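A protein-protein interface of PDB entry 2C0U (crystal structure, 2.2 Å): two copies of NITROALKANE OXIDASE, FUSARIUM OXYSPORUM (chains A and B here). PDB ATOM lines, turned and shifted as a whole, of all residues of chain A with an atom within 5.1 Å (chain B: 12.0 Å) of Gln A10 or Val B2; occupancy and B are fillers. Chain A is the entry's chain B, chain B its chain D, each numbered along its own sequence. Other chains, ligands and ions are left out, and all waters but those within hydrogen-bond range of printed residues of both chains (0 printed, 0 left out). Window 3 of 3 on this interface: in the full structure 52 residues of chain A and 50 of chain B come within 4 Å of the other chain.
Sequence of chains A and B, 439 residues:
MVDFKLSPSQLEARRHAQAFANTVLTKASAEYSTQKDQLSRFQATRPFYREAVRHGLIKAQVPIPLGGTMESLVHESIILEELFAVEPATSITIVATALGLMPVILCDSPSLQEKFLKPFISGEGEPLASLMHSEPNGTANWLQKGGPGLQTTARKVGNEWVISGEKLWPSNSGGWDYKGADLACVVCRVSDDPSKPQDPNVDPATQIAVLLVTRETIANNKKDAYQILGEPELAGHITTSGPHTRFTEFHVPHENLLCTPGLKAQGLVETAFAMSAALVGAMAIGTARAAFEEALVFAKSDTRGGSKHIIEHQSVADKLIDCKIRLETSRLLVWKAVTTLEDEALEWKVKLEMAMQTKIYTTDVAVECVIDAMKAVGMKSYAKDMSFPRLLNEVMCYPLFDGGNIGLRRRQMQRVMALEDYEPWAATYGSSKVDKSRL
CG1 of Val B2 touches O of Phe A4, 3.8 Å away.
Phe A4 touches Trp B335 (CE1 to C, 3.9 Å).
Phe A4 touches Lys B336.
Phe A4 touches Thr B339.
Val B2 touches Leu A6.
Gln A10 touches Val B2.
Arg A14 touches Tyr B429 (NE to CD1, 3.2 Å).
CG1 of Val A74 touches CG2 of Val B2 (3.9 Å).
Phe B4 touches Trp A335 (CE1 to O, 3.8 Å).
OG1 of Thr A339 touches CE1 of Phe B4 (3.7 Å).
The side-chain amino group (NZ) of Lys A5 lies within salt-bridge range of the side-chain carboxylate (OD2) of Asp B343 (2.8 Å).
N of Asp A3 lies within hydrogen-bond range of O of Asp B3.
Hydrophobic or aromatic side chains of chain B that line the printed part of chain A: Val B2, Phe B4 and Tyr B429.
Of the 18 printed residues of chain A, 9 touch a printed residue of chain B.
Among the printed residues, Asp or Glu carboxylates within 4 Å of a Lys or Arg side-chain nitrogen of the other chain: Lys A5 with Asp B343.
Asp A3 touches its own counterpart, Asp B3.
Phe B4 touches its own counterpart, Phe A4.
Phe A4 touches Trp B335, and with the chains exchanged Trp A335 touches Phe B4.
Phe A4 touches Thr B339, and with the chains exchanged Thr A339 touches Phe B4.
Of chain B, only Val B2 and Asp B3 come within 4 Å of Asp A3.
Of chain B, only Val B2, Phe B4, Trp B335, Lys B336 and Thr B339 come within 4 Å of Phe A4.
Printed residues of chain B within 4 Å of Lys A5: Val B2 (3.6 Å) and Asp B343 (2.8 Å).
Leu A6 touches just these residues of chain B: Val B2 (3.7 Å), Thr B428 (3.9 Å) and Tyr B429 (3.5 Å).
No residue of chain B comes within 4 Å of Pro A8.
No residue of chain B comes within 4 Å of Ser A9.
Of chain B, only Val B2 comes within 4 Å of Gln A10.
No residue of chain B comes within 4 Å of Glu A12.
No residue of chain B comes within 4 Å of Ser A72.
Of chain B, only Val B2 comes within 4 Å of Val A74.
No residue of chain B comes within 4 Å of His A75.
No residue of chain B comes within 4 Å of Ile A78.
Thr A339 touches just one residue of chain B: Phe B4 (3.7 Å).
Val B2 touches just these residues of chain A: Asp A3, Phe A4, Lys A5, Leu A6, Gln A10 and Val A74.
Printed residues of chain A within 4 Å of Asp B3: Asp A3.
Leu B332 touches none of the printed residues of chain A.
Of the printed residues of chain A, Trp B335 touches Phe A4.
Of the printed residues of chain A, Thr B339 touches Phe A4.
Ala B427 touches none of the printed residues of chain A.
The nearest printed residue of chain A that does not touch Thr B428 is Phe A4 (4.8 Å).
The side-chain amino group (NZ) of Lys B336 sits close to the backbone carbonyl oxygen (O) of Ala B427, at 3.5 Å.
The side-chain carboxylate of Asp A3 sits close to the backbone NH of Lys A5, at 3.2 Å.
The backbone NH of Ser A7 lies within hydrogen-bond range of the side-chain amide oxygen of Gln A10.
The backbone carbonyl oxygen of Lys B336 lies within hydrogen-bond range of the side-chain hydroxyl of Thr B340, at 2.8 Å.
O of Lys B336 sits at hydrogen-bond distance from OG1 of Thr B339 (2.7 Å).
OG1 of Thr B428 lies within hydrogen-bond range of NZ of Lys B336 (3.0 Å).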
ATOM      1  N   ASP A   3      16.318  29.252 -27.375  1.00  0.00           N
ATOM      2  CA  ASP A   3      16.737  28.235 -26.420  1.00  0.00           C
ATOM      3  C   ASP A   3      15.541  27.615 -25.711  1.00  0.00           C
ATOM      4  O   ASP A   3      14.710  28.327 -25.145  1.00  0.00           O
ATOM      5  CB  ASP A   3      17.683  28.855 -25.389  1.00  0.00           C
ATOM      6  CG  ASP A   3      17.997  27.912 -24.251  1.00  0.00           C
ATOM      7  OD1 ASP A   3      18.559  26.829 -24.519  1.00  0.00           O
ATOM      8  OD2 ASP A   3      17.678  28.248 -23.089  1.00  0.00           O
ATOM      9  N   PHE A   4      15.457  26.288 -25.739  1.00  0.00           N
ATOM     10  CA  PHE A   4      14.354  25.583 -25.093  1.00  0.00           C
ATOM     11  C   PHE A   4      14.833  24.807 -23.876  1.00  0.00           C
ATOM     12  O   PHE A   4      14.098  24.001 -23.311  1.00  0.00           O
ATOM     13  CB  PHE A   4      13.676  24.624 -26.077  1.00  0.00           C
ATOM     14  CG  PHE A   4      13.098  25.305 -27.288  1.00  0.00           C
ATOM     15  CD1 PHE A   4      13.893  25.571 -28.399  1.00  0.00           C
ATOM     16  CD2 PHE A   4      11.762  25.703 -27.307  1.00  0.00           C
ATOM     17  CE1 PHE A   4      13.367  26.227 -29.512  1.00  0.00           C
ATOM     18  CE2 PHE A   4      11.224  26.362 -28.415  1.00  0.00           C
ATOM     19  CZ  PHE A   4      12.025  26.624 -29.518  1.00  0.00           C
ATOM     20  N   LYS A   5      16.075  25.060 -23.482  1.00  0.00           N
ATOM     21  CA  LYS A   5      16.665  24.405 -22.325  1.00  0.00           C
ATOM     22  C   LYS A   5      16.043  24.952 -21.039  1.00  0.00           C
ATOM     23  O   LYS A   5      16.062  26.158 -20.794  1.00  0.00           O
ATOM     24  CB  LYS A   5      18.177  24.646 -22.314  1.00  0.00           C
ATOM     25  CG  LYS A   5      19.024  23.421 -22.629  1.00  0.00           C
ATOM     26  CD  LYS A   5      18.978  22.413 -21.490  1.00  0.00           C
ATOM     27  CE  LYS A   5      19.866  21.209 -21.773  1.00  0.00           C
ATOM     28  NZ  LYS A   5      19.418  20.445 -22.972  1.00  0.00           N
ATOM     29  N   LEU A   6      15.486  24.068 -20.221  1.00  0.00           N
ATOM     30  CA  LEU A   6      14.882  24.491 -18.967  1.00  0.00           C
ATOM     31  C   LEU A   6      15.933  24.711 -17.885  1.00  0.00           C
ATOM     32  O   LEU A   6      16.825  23.886 -17.692  1.00  0.00           O
ATOM     33  CB  LEU A   6      13.870  23.455 -18.484  1.00  0.00           C
ATOM     34  CG  LEU A   6      12.544  23.403 -19.238  1.00  0.00           C
ATOM     35  CD1 LEU A   6      11.661  22.344 -18.611  1.00  0.00           C
ATOM     36  CD2 LEU A   6      11.862  24.760 -19.178  1.00  0.00           C
ATOM     37  N   SER A   7      15.819  25.829 -17.180  1.00  0.00           N
ATOM     38  CA  SER A   7      16.753  26.154 -16.112  1.00  0.00           C
ATOM     39  C   SER A   7      16.488  25.251 -14.915  1.00  0.00           C
ATOM     40  O   SER A   7      15.461  24.573 -14.848  1.00  0.00           O
ATOM     41  CB  SER A   7      16.594  27.617 -15.689  1.00  0.00           C
ATOM     42  OG  SER A   7      15.366  27.819 -15.002  1.00  0.00           O
ATOM     43  N   PRO A   8      17.419  25.226 -13.955  1.00  0.00           N
ATOM     44  CA  PRO A   8      17.262  24.395 -12.761  1.00  0.00           C
ATOM     45  C   PRO A   8      16.011  24.752 -11.970  1.00  0.00           C
ATOM     46  O   PRO A   8      15.351  23.871 -11.421  1.00  0.00           O
ATOM     47  CB  PRO A   8      18.540  24.671 -11.982  1.00  0.00           C
ATOM     48  CG  PRO A   8      19.541  24.904 -13.082  1.00  0.00           C
ATOM     49  CD  PRO A   8      18.772  25.808 -14.011  1.00  0.00           C
ATOM     50  N   SER A   9      15.689  26.042 -11.909  1.00  0.00           N
ATOM     51  CA  SER A   9      14.506  26.497 -11.175  1.00  0.00           C
ATOM     52  C   SER A   9      13.212  26.026 -11.835  1.00  0.00           C
ATOM     53  O   SER A   9      12.252  25.673 -11.145  1.00  0.00           O
ATOM     54  CB  SER A   9      14.504  28.026 -11.052  1.00  0.00           C
ATOM     55  OG  SER A   9      14.606  28.649 -12.316  1.00  0.00           O
ATOM     56  N   GLN A  10      13.183  26.024 -13.166  1.00  0.00           N
ATOM     57  CA  GLN A  10      12.003  25.568 -13.906  1.00  0.00           C
ATOM     58  C   GLN A  10      11.848  24.062 -13.724  1.00  0.00           C
ATOM     59  O   GLN A  10      10.754  23.586 -13.430  1.00  0.00           O
ATOM     60  CB  GLN A  10      12.133  25.907 -15.398  1.00  0.00           C
ATOM     61  CG  GLN A  10      12.283  27.393 -15.627  1.00  0.00           C
ATOM     62  CD  GLN A  10      12.635  27.764 -17.048  1.00  0.00           C
ATOM     63  OE1 GLN A  10      13.547  27.194 -17.655  1.00  0.00           O
ATOM     64  NE2 GLN A  10      11.931  28.751 -17.581  1.00  0.00           N
ATOM     65  N   LEU A  11      12.947  23.323 -13.886  1.00  0.00           N
ATOM     66  CA  LEU A  11      12.934  21.866 -13.727  1.00  0.00           C
ATOM     67  C   LEU A  11      12.502  21.532 -12.305  1.00  0.00           C
ATOM     68  O   LEU A  11      11.805  20.553 -12.058  1.00  0.00           O
ATOM     69  CB  LEU A  11      14.325  21.281 -14.005  1.00  0.00           C
ATOM     70  CG  LEU A  11      14.846  21.429 -15.439  1.00  0.00           C
ATOM     71  CD1 LEU A  11      16.328  21.135 -15.469  1.00  0.00           C
ATOM     72  CD2 LEU A  11      14.096  20.495 -16.373  1.00  0.00           C
ATOM     73  N   GLU A  12      12.911  22.373 -11.370  1.00  0.00           N
ATOM     74  CA  GLU A  12      12.558  22.192  -9.974  1.00  0.00           C
ATOM     75  C   GLU A  12      11.062  22.484  -9.750  1.00  0.00           C
ATOM     76  O   GLU A  12      10.403  21.880  -8.894  1.00  0.00           O
ATOM     77  CB  GLU A  12      13.418  23.134  -9.140  1.00  0.00           C
ATOM     78  CG  GLU A  12      13.891  22.545  -7.844  1.00  0.00           C
ATOM     79  CD  GLU A  12      12.762  22.345  -6.871  1.00  0.00           C
ATOM     80  OE1 GLU A  12      12.142  23.356  -6.480  1.00  0.00           O
ATOM     81  OE2 GLU A  12      12.495  21.181  -6.498  1.00  0.00           O
ATOM     82  N   ALA A  13      10.529  23.421 -10.529  1.00  0.00           N
ATOM     83  CA  ALA A  13       9.123  23.791 -10.420  1.00  0.00           C
ATOM     84  C   ALA A  13       8.258  22.609 -10.855  1.00  0.00           C
ATOM     85  O   ALA A  13       7.244  22.291 -10.235  1.00  0.00           O
ATOM     86  CB  ALA A  13       8.842  25.024 -11.291  1.00  0.00           C
ATOM     87  N   ARG A  14       8.675  21.941 -11.920  1.00  0.00           N
ATOM     88  CA  ARG A  14       7.930  20.796 -12.415  1.00  0.00           C
ATOM     89  C   ARG A  14       7.929  19.692 -11.359  1.00  0.00           C
ATOM     90  O   ARG A  14       6.878  19.132 -11.016  1.00  0.00           O
ATOM     91  CB  ARG A  14       8.564  20.302 -13.720  1.00  0.00           C
ATOM     92  CG  ARG A  14       7.890  19.087 -14.332  1.00  0.00           C
ATOM     93  CD  ARG A  14       8.390  18.841 -15.749  1.00  0.00           C
ATOM     94  NE  ARG A  14       7.652  17.770 -16.416  1.00  0.00           N
ATOM     95  CZ  ARG A  14       8.005  16.490 -16.408  1.00  0.00           C
ATOM     96  NH1 ARG A  14       9.101  16.102 -15.771  1.00  0.00           N
ATOM     97  NH2 ARG A  14       7.258  15.598 -17.040  1.00  0.00           N
ATOM     98  N   SER A  72       8.263  33.137 -12.913  1.00  0.00           N
ATOM     99  CA  SER A  72       7.980  33.560 -14.282  1.00  0.00           C
ATOM    100  C   SER A  72       6.732  32.851 -14.771  1.00  0.00           C
ATOM    101  O   SER A  72       6.261  31.905 -14.137  1.00  0.00           O
ATOM    102  CB  SER A  72       9.138  33.225 -15.224  1.00  0.00           C
ATOM    103  OG  SER A  72       9.002  31.912 -15.742  1.00  0.00           O
ATOM    104  N   VAL A  74       6.558  31.092 -17.449  1.00  0.00           N
ATOM    105  CA  VAL A  74       6.978  29.791 -17.958  1.00  0.00           C
ATOM    106  C   VAL A  74       6.929  28.777 -16.811  1.00  0.00           C
ATOM    107  O   VAL A  74       6.509  27.635 -17.010  1.00  0.00           O
ATOM    108  CB  VAL A  74       8.399  29.837 -18.499  1.00  0.00           C
ATOM    109  CG1 VAL A  74       8.810  28.470 -18.979  1.00  0.00           C
ATOM    110  CG2 VAL A  74       8.483  30.831 -19.621  1.00  0.00           C
ATOM    111  N   HIS A  75       7.363  29.185 -15.614  1.00  0.00           N
ATOM    112  CA  HIS A  75       7.316  28.293 -14.451  1.00  0.00           C
ATOM    113  C   HIS A  75       5.854  27.951 -14.177  1.00  0.00           C
ATOM    114  O   HIS A  75       5.512  26.801 -13.895  1.00  0.00           O
ATOM    115  CB  HIS A  75       7.891  28.950 -13.179  1.00  0.00           C
ATOM    116  CG  HIS A  75       9.361  29.209 -13.229  1.00  0.00           C
ATOM    117  ND1 HIS A  75       9.934  30.079 -14.133  1.00  0.00           N
ATOM    118  CD2 HIS A  75      10.387  28.694 -12.504  1.00  0.00           C
ATOM    119  CE1 HIS A  75      11.244  30.086 -13.966  1.00  0.00           C
ATOM    120  NE2 HIS A  75      11.544  29.256 -12.989  1.00  0.00           N
ATOM    121  N   ILE A  78       4.590  25.512 -16.739  1.00  0.00           N
ATOM    122  CA  ILE A  78       5.102  24.183 -16.436  1.00  0.00           C
ATOM    123  C   ILE A  78       4.357  23.573 -15.266  1.00  0.00           C
ATOM    124  O   ILE A  78       4.046  22.384 -15.273  1.00  0.00           O
ATOM    125  CB  ILE A  78       6.593  24.238 -16.093  1.00  0.00           C
ATOM    126  CG1 ILE A  78       7.378  24.675 -17.323  1.00  0.00           C
ATOM    127  CG2 ILE A  78       7.070  22.874 -15.623  1.00  0.00           C
ATOM    128  CD1 ILE A  78       8.852  24.856 -17.083  1.00  0.00           C
ATOM    129  N   TRP A 335       4.612  28.557 -24.280  1.00  0.00           N
ATOM    130  CA  TRP A 335       5.873  29.096 -23.823  1.00  0.00           C
ATOM    131  C   TRP A 335       6.215  30.369 -24.580  1.00  0.00           C
ATOM    132  O   TRP A 335       6.688  31.337 -23.992  1.00  0.00           O
ATOM    133  CB  TRP A 335       6.980  28.062 -23.997  1.00  0.00           C
ATOM    134  CG  TRP A 335       6.901  26.929 -23.028  1.00  0.00           C
ATOM    135  CD1 TRP A 335       5.880  26.641 -22.166  1.00  0.00           C
ATOM    136  CD2 TRP A 335       7.907  25.938 -22.808  1.00  0.00           C
ATOM    137  NE1 TRP A 335       6.192  25.526 -21.417  1.00  0.00           N
ATOM    138  CE2 TRP A 335       7.434  25.078 -21.792  1.00  0.00           C
ATOM    139  CE3 TRP A 335       9.166  25.695 -23.370  1.00  0.00           C
ATOM    140  CZ2 TRP A 335       8.177  23.989 -21.328  1.00  0.00           C
ATOM    141  CZ3 TRP A 335       9.910  24.613 -22.905  1.00  0.00           C
ATOM    142  CH2 TRP A 335       9.410  23.775 -21.895  1.00  0.00           C
ATOM    143  N   THR A 339       6.267  34.033 -22.830  1.00  0.00           N
ATOM    144  CA  THR A 339       7.552  34.698 -22.998  1.00  0.00           C
ATOM    145  C   THR A 339       7.341  36.056 -23.672  1.00  0.00           C
ATOM    146  O   THR A 339       7.977  37.052 -23.311  1.00  0.00           O
ATOM    147  CB  THR A 339       8.523  33.843 -23.859  1.00  0.00           C
ATOM    148  OG1 THR A 339       9.022  32.749 -23.082  1.00  0.00           O
ATOM    149  CG2 THR A 339       9.695  34.676 -24.325  1.00  0.00           C
ATOM    150  N   VAL B   2      14.134  29.567 -20.784  1.00  0.00           N
ATOM    151  CA  VAL B   2      13.827  29.413 -22.233  1.00  0.00           C
ATOM    152  C   VAL B   2      13.549  30.776 -22.848  1.00  0.00           C
ATOM    153  O   VAL B   2      12.929  31.633 -22.218  1.00  0.00           O
ATOM    154  CB  VAL B   2      12.592  28.520 -22.448  1.00  0.00           C
ATOM    155  CG1 VAL B   2      12.802  27.183 -21.783  1.00  0.00           C
ATOM    156  CG2 VAL B   2      11.364  29.188 -21.882  1.00  0.00           C
ATOM    157  N   ASP B   3      14.019  30.975 -24.076  1.00  0.00           N
ATOM    158  CA  ASP B   3      13.816  32.238 -24.780  1.00  0.00           C
ATOM    159  C   ASP B   3      13.722  31.985 -26.274  1.00  0.00           C
ATOM    160  O   ASP B   3      14.095  30.917 -26.753  1.00  0.00           O
ATOM    161  CB  ASP B   3      14.976  33.204 -24.520  1.00  0.00           C
ATOM    162  CG  ASP B   3      16.204  32.882 -25.359  1.00  0.00           C
ATOM    163  OD1 ASP B   3      16.834  31.833 -25.117  1.00  0.00           O
ATOM    164  OD2 ASP B   3      16.536  33.679 -26.268  1.00  0.00           O
ATOM    165  N   PHE B   4      13.243  32.979 -27.010  1.00  0.00           N
ATOM    166  CA  PHE B   4      13.111  32.844 -28.451  1.00  0.00           C
ATOM    167  C   PHE B   4      13.781  34.005 -29.167  1.00  0.00           C
ATOM    168  O   PHE B   4      13.765  34.076 -30.396  1.00  0.00           O
ATOM    169  CB  PHE B   4      11.633  32.783 -28.844  1.00  0.00           C
ATOM    170  CG  PHE B   4      10.866  31.703 -28.139  1.00  0.00           C
ATOM    171  CD1 PHE B   4      10.486  31.856 -26.812  1.00  0.00           C
ATOM    172  CD2 PHE B   4      10.545  30.520 -28.797  1.00  0.00           C
ATOM    173  CE1 PHE B   4       9.797  30.846 -26.146  1.00  0.00           C
ATOM    174  CE2 PHE B   4       9.855  29.500 -28.143  1.00  0.00           C
ATOM    175  CZ  PHE B   4       9.481  29.665 -26.814  1.00  0.00           C
ATOM    176  N   LYS B   5      14.372  34.912 -28.395  1.00  0.00           N
ATOM    177  CA  LYS B   5      15.040  36.080 -28.964  1.00  0.00           C
ATOM    178  C   LYS B   5      16.185  35.672 -29.890  1.00  0.00           C
ATOM    179  O   LYS B   5      16.971  34.778 -29.580  1.00  0.00           O
ATOM    180  CB  LYS B   5      15.560  36.987 -27.842  1.00  0.00           C
ATOM    181  CG  LYS B   5      16.083  38.351 -28.301  1.00  0.00           C
ATOM    182  CD  LYS B   5      15.005  39.167 -29.015  1.00  0.00           C
ATOM    183  CE  LYS B   5      15.073  38.994 -30.529  1.00  0.00           C
ATOM    184  NZ  LYS B   5      13.875  39.531 -31.237  1.00  0.00           N
ATOM    185  N   LEU B   6      16.264  36.335 -31.036  1.00  0.00           N
ATOM    186  CA  LEU B   6      17.294  36.038 -32.011  1.00  0.00           C
ATOM    187  C   LEU B   6      18.563  36.820 -31.729  1.00  0.00           C
ATOM    188  O   LEU B   6      18.510  37.997 -31.377  1.00  0.00           O
ATOM    189  CB  LEU B   6      16.795  36.364 -33.418  1.00  0.00           C
ATOM    190  CG  LEU B   6      15.563  35.599 -33.907  1.00  0.00           C
ATOM    191  CD1 LEU B   6      15.174  36.119 -35.269  1.00  0.00           C
ATOM    192  CD2 LEU B   6      15.852  34.111 -33.981  1.00  0.00           C
ATOM    193  N   LEU B 332       7.725  27.563 -34.589  1.00  0.00           N
ATOM    194  CA  LEU B 332       8.188  27.169 -33.271  1.00  0.00           C
ATOM    195  C   LEU B 332       8.638  25.714 -33.275  1.00  0.00           C
ATOM    196  O   LEU B 332       9.650  25.367 -32.669  1.00  0.00           O
ATOM    197  CB  LEU B 332       7.086  27.355 -32.235  1.00  0.00           C
ATOM    198  CG  LEU B 332       6.644  28.811 -32.031  1.00  0.00           C
ATOM    199  CD1 LEU B 332       5.599  28.873 -30.947  1.00  0.00           C
ATOM    200  CD2 LEU B 332       7.832  29.657 -31.649  1.00  0.00           C
ATOM    201  N   TRP B 335      12.030  25.363 -35.145  1.00  0.00           N
ATOM    202  CA  TRP B 335      13.114  25.847 -34.302  1.00  0.00           C
ATOM    203  C   TRP B 335      13.407  24.836 -33.200  1.00  0.00           C
ATOM    204  O   TRP B 335      14.562  24.519 -32.937  1.00  0.00           O
ATOM    205  CB  TRP B 335      12.746  27.214 -33.715  1.00  0.00           C
ATOM    206  CG  TRP B 335      12.822  28.347 -34.719  1.00  0.00           C
ATOM    207  CD1 TRP B 335      13.010  28.244 -36.070  1.00  0.00           C
ATOM    208  CD2 TRP B 335      12.761  29.748 -34.429  1.00  0.00           C
ATOM    209  NE1 TRP B 335      13.079  29.494 -36.637  1.00  0.00           N
ATOM    210  CE2 TRP B 335      12.929  30.436 -35.653  1.00  0.00           C
ATOM    211  CE3 TRP B 335      12.585  30.490 -33.257  1.00  0.00           C
ATOM    212  CZ2 TRP B 335      12.927  31.834 -35.734  1.00  0.00           C
ATOM    213  CZ3 TRP B 335      12.583  31.879 -33.336  1.00  0.00           C
ATOM    214  CH2 TRP B 335      12.753  32.535 -34.566  1.00  0.00           C
ATOM    215  N   LYS B 336      12.359  24.322 -32.567  1.00  0.00           N
ATOM    216  CA  LYS B 336      12.535  23.323 -31.528  1.00  0.00           C
ATOM    217  C   LYS B 336      13.255  22.093 -32.114  1.00  0.00           C
ATOM    218  O   LYS B 336      14.195  21.570 -31.518  1.00  0.00           O
ATOM    219  CB  LYS B 336      11.172  22.906 -30.972  1.00  0.00           C
ATOM    220  CG  LYS B 336      11.227  21.803 -29.921  1.00  0.00           C
ATOM    221  CD  LYS B 336      12.084  22.210 -28.721  1.00  0.00           C
ATOM    222  CE  LYS B 336      12.255  21.069 -27.725  1.00  0.00           C
ATOM    223  NZ  LYS B 336      10.943  20.650 -27.175  1.00  0.00           N
ATOM    224  N   THR B 339      17.036  22.735 -32.969  1.00  0.00           N
ATOM    225  CA  THR B 339      17.829  22.843 -31.753  1.00  0.00           C
ATOM    226  C   THR B 339      17.986  21.451 -31.139  1.00  0.00           C
ATOM    227  O   THR B 339      19.082  21.063 -30.740  1.00  0.00           O
ATOM    228  CB  THR B 339      17.176  23.798 -30.718  1.00  0.00           C
ATOM    229  OG1 THR B 339      15.878  23.312 -30.365  1.00  0.00           O
ATOM    230  CG2 THR B 339      17.045  25.211 -31.289  1.00  0.00           C
ATOM    231  N   THR B 340      16.892  20.699 -31.073  1.00  0.00           N
ATOM    232  CA  THR B 340      16.929  19.354 -30.510  1.00  0.00           C
ATOM    233  C   THR B 340      17.949  18.493 -31.254  1.00  0.00           C
ATOM    234  O   THR B 340      18.634  17.663 -30.657  1.00  0.00           O
ATOM    235  CB  THR B 340      15.554  18.681 -30.608  1.00  0.00           C
ATOM    236  OG1 THR B 340      14.611  19.407 -29.811  1.00  0.00           O
ATOM    237  CG2 THR B 340      15.620  17.257 -30.106  1.00  0.00           C
ATOM    238  N   ASP B 343      21.347  19.174 -29.901  1.00  0.00           N
ATOM    239  CA  ASP B 343      21.542  18.897 -28.480  1.00  0.00           C
ATOM    240  C   ASP B 343      22.164  17.510 -28.316  1.00  0.00           C
ATOM    241  O   ASP B 343      21.455  16.507 -28.218  1.00  0.00           O
ATOM    242  CB  ASP B 343      20.199  18.943 -27.747  1.00  0.00           C
ATOM    243  CG  ASP B 343      20.353  18.859 -26.241  1.00  0.00           C
ATOM    244  OD1 ASP B 343      21.346  18.262 -25.780  1.00  0.00           O
ATOM    245  OD2 ASP B 343      19.473  19.377 -25.516  1.00  0.00           O
ATOM    246  N   TRP B 425       8.386  12.985 -23.798  1.00  0.00           N
ATOM    247  CA  TRP B 425       8.839  14.357 -23.611  1.00  0.00           C
ATOM    248  C   TRP B 425      10.319  14.526 -23.292  1.00  0.00           C
ATOM    249  O   TRP B 425      10.713  15.503 -22.655  1.00  0.00           O
ATOM    250  CB  TRP B 425       7.991  14.981 -22.517  1.00  0.00           C
ATOM    251  CG  TRP B 425       6.569  14.532 -22.618  1.00  0.00           C
ATOM    252  CD1 TRP B 425       5.902  13.731 -21.751  1.00  0.00           C
ATOM    253  CD2 TRP B 425       5.629  14.878 -23.657  1.00  0.00           C
ATOM    254  NE1 TRP B 425       4.600  13.552 -22.164  1.00  0.00           N
ATOM    255  CE2 TRP B 425       4.408  14.247 -23.332  1.00  0.00           C
ATOM    256  CE3 TRP B 425       5.700  15.657 -24.819  1.00  0.00           C
ATOM    257  CZ2 TRP B 425       3.263  14.371 -24.126  1.00  0.00           C
ATOM    258  CZ3 TRP B 425       4.551  15.784 -25.614  1.00  0.00           C
ATOM    259  CH2 TRP B 425       3.355  15.141 -25.256  1.00  0.00           C
ATOM    260  N   ALA B 426      11.141  13.594 -23.755  1.00  0.00           N
ATOM    261  CA  ALA B 426      12.569  13.659 -23.481  1.00  0.00           C
ATOM    262  C   ALA B 426      13.193  14.928 -24.026  1.00  0.00           C
ATOM    263  O   ALA B 426      14.109  15.488 -23.416  1.00  0.00           O
ATOM    264  CB  ALA B 426      13.274  12.444 -24.067  1.00  0.00           C
ATOM    265  N   ALA B 427      12.690  15.391 -25.166  1.00  0.00           N
ATOM    266  CA  ALA B 427      13.221  16.593 -25.800  1.00  0.00           C
ATOM    267  C   ALA B 427      12.807  17.867 -25.091  1.00  0.00           C
ATOM    268  O   ALA B 427      13.359  18.931 -25.351  1.00  0.00           O
ATOM    269  CB  ALA B 427      12.776  16.652 -27.264  1.00  0.00           C
ATOM    270  N   THR B 428      11.842  17.766 -24.188  1.00  0.00           N
ATOM    271  CA  THR B 428      11.381  18.950 -23.478  1.00  0.00           C
ATOM    272  C   THR B 428      11.796  18.956 -22.006  1.00  0.00           C
ATOM    273  O   THR B 428      12.472  19.872 -21.539  1.00  0.00           O
ATOM    274  CB  THR B 428       9.843  19.079 -23.559  1.00  0.00           C
ATOM    275  OG1 THR B 428       9.456  19.359 -24.909  1.00  0.00           O
ATOM    276  CG2 THR B 428       9.362  20.194 -22.663  1.00  0.00           C
ATOM    277  N   TYR B 429      11.380  17.927 -21.285  1.00  0.00           N
ATOM    278  CA  TYR B 429      11.677  17.820 -19.872  1.00  0.00           C
ATOM    279  C   TYR B 429      12.836  16.868 -19.596  1.00  0.00           C
ATOM    280  O   TYR B 429      12.929  16.290 -18.513  1.00  0.00           O
ATOM    281  CB  TYR B 429      10.421  17.352 -19.143  1.00  0.00           C
ATOM    282  CG  TYR B 429       9.275  18.331 -19.246  1.00  0.00           C
ATOM    283  CD1 TYR B 429       7.993  17.906 -19.601  1.00  0.00           C
ATOM    284  CD2 TYR B 429       9.461  19.679 -18.945  1.00  0.00           C
ATOM    285  CE1 TYR B 429       6.924  18.801 -19.647  1.00  0.00           C
ATOM    286  CE2 TYR B 429       8.407  20.580 -18.988  1.00  0.00           C
ATOM    287  CZ  TYR B 429       7.142  20.140 -19.332  1.00  0.00           C
ATOM    288  OH  TYR B 429       6.095  21.035 -19.322  1.00  0.00           O
ATOM    289  N   GLY B 430      13.717  16.711 -20.579  1.00  0.00           N
ATOM    290  CA  GLY B 430      14.853  15.822 -20.427  1.00  0.00           C
ATOM    291  C   GLY B 430      14.475  14.370 -20.193  1.00  0.00           C
ATOM    292  O   GLY B 430      13.302  14.030 -20.026  1.00  0.00           O
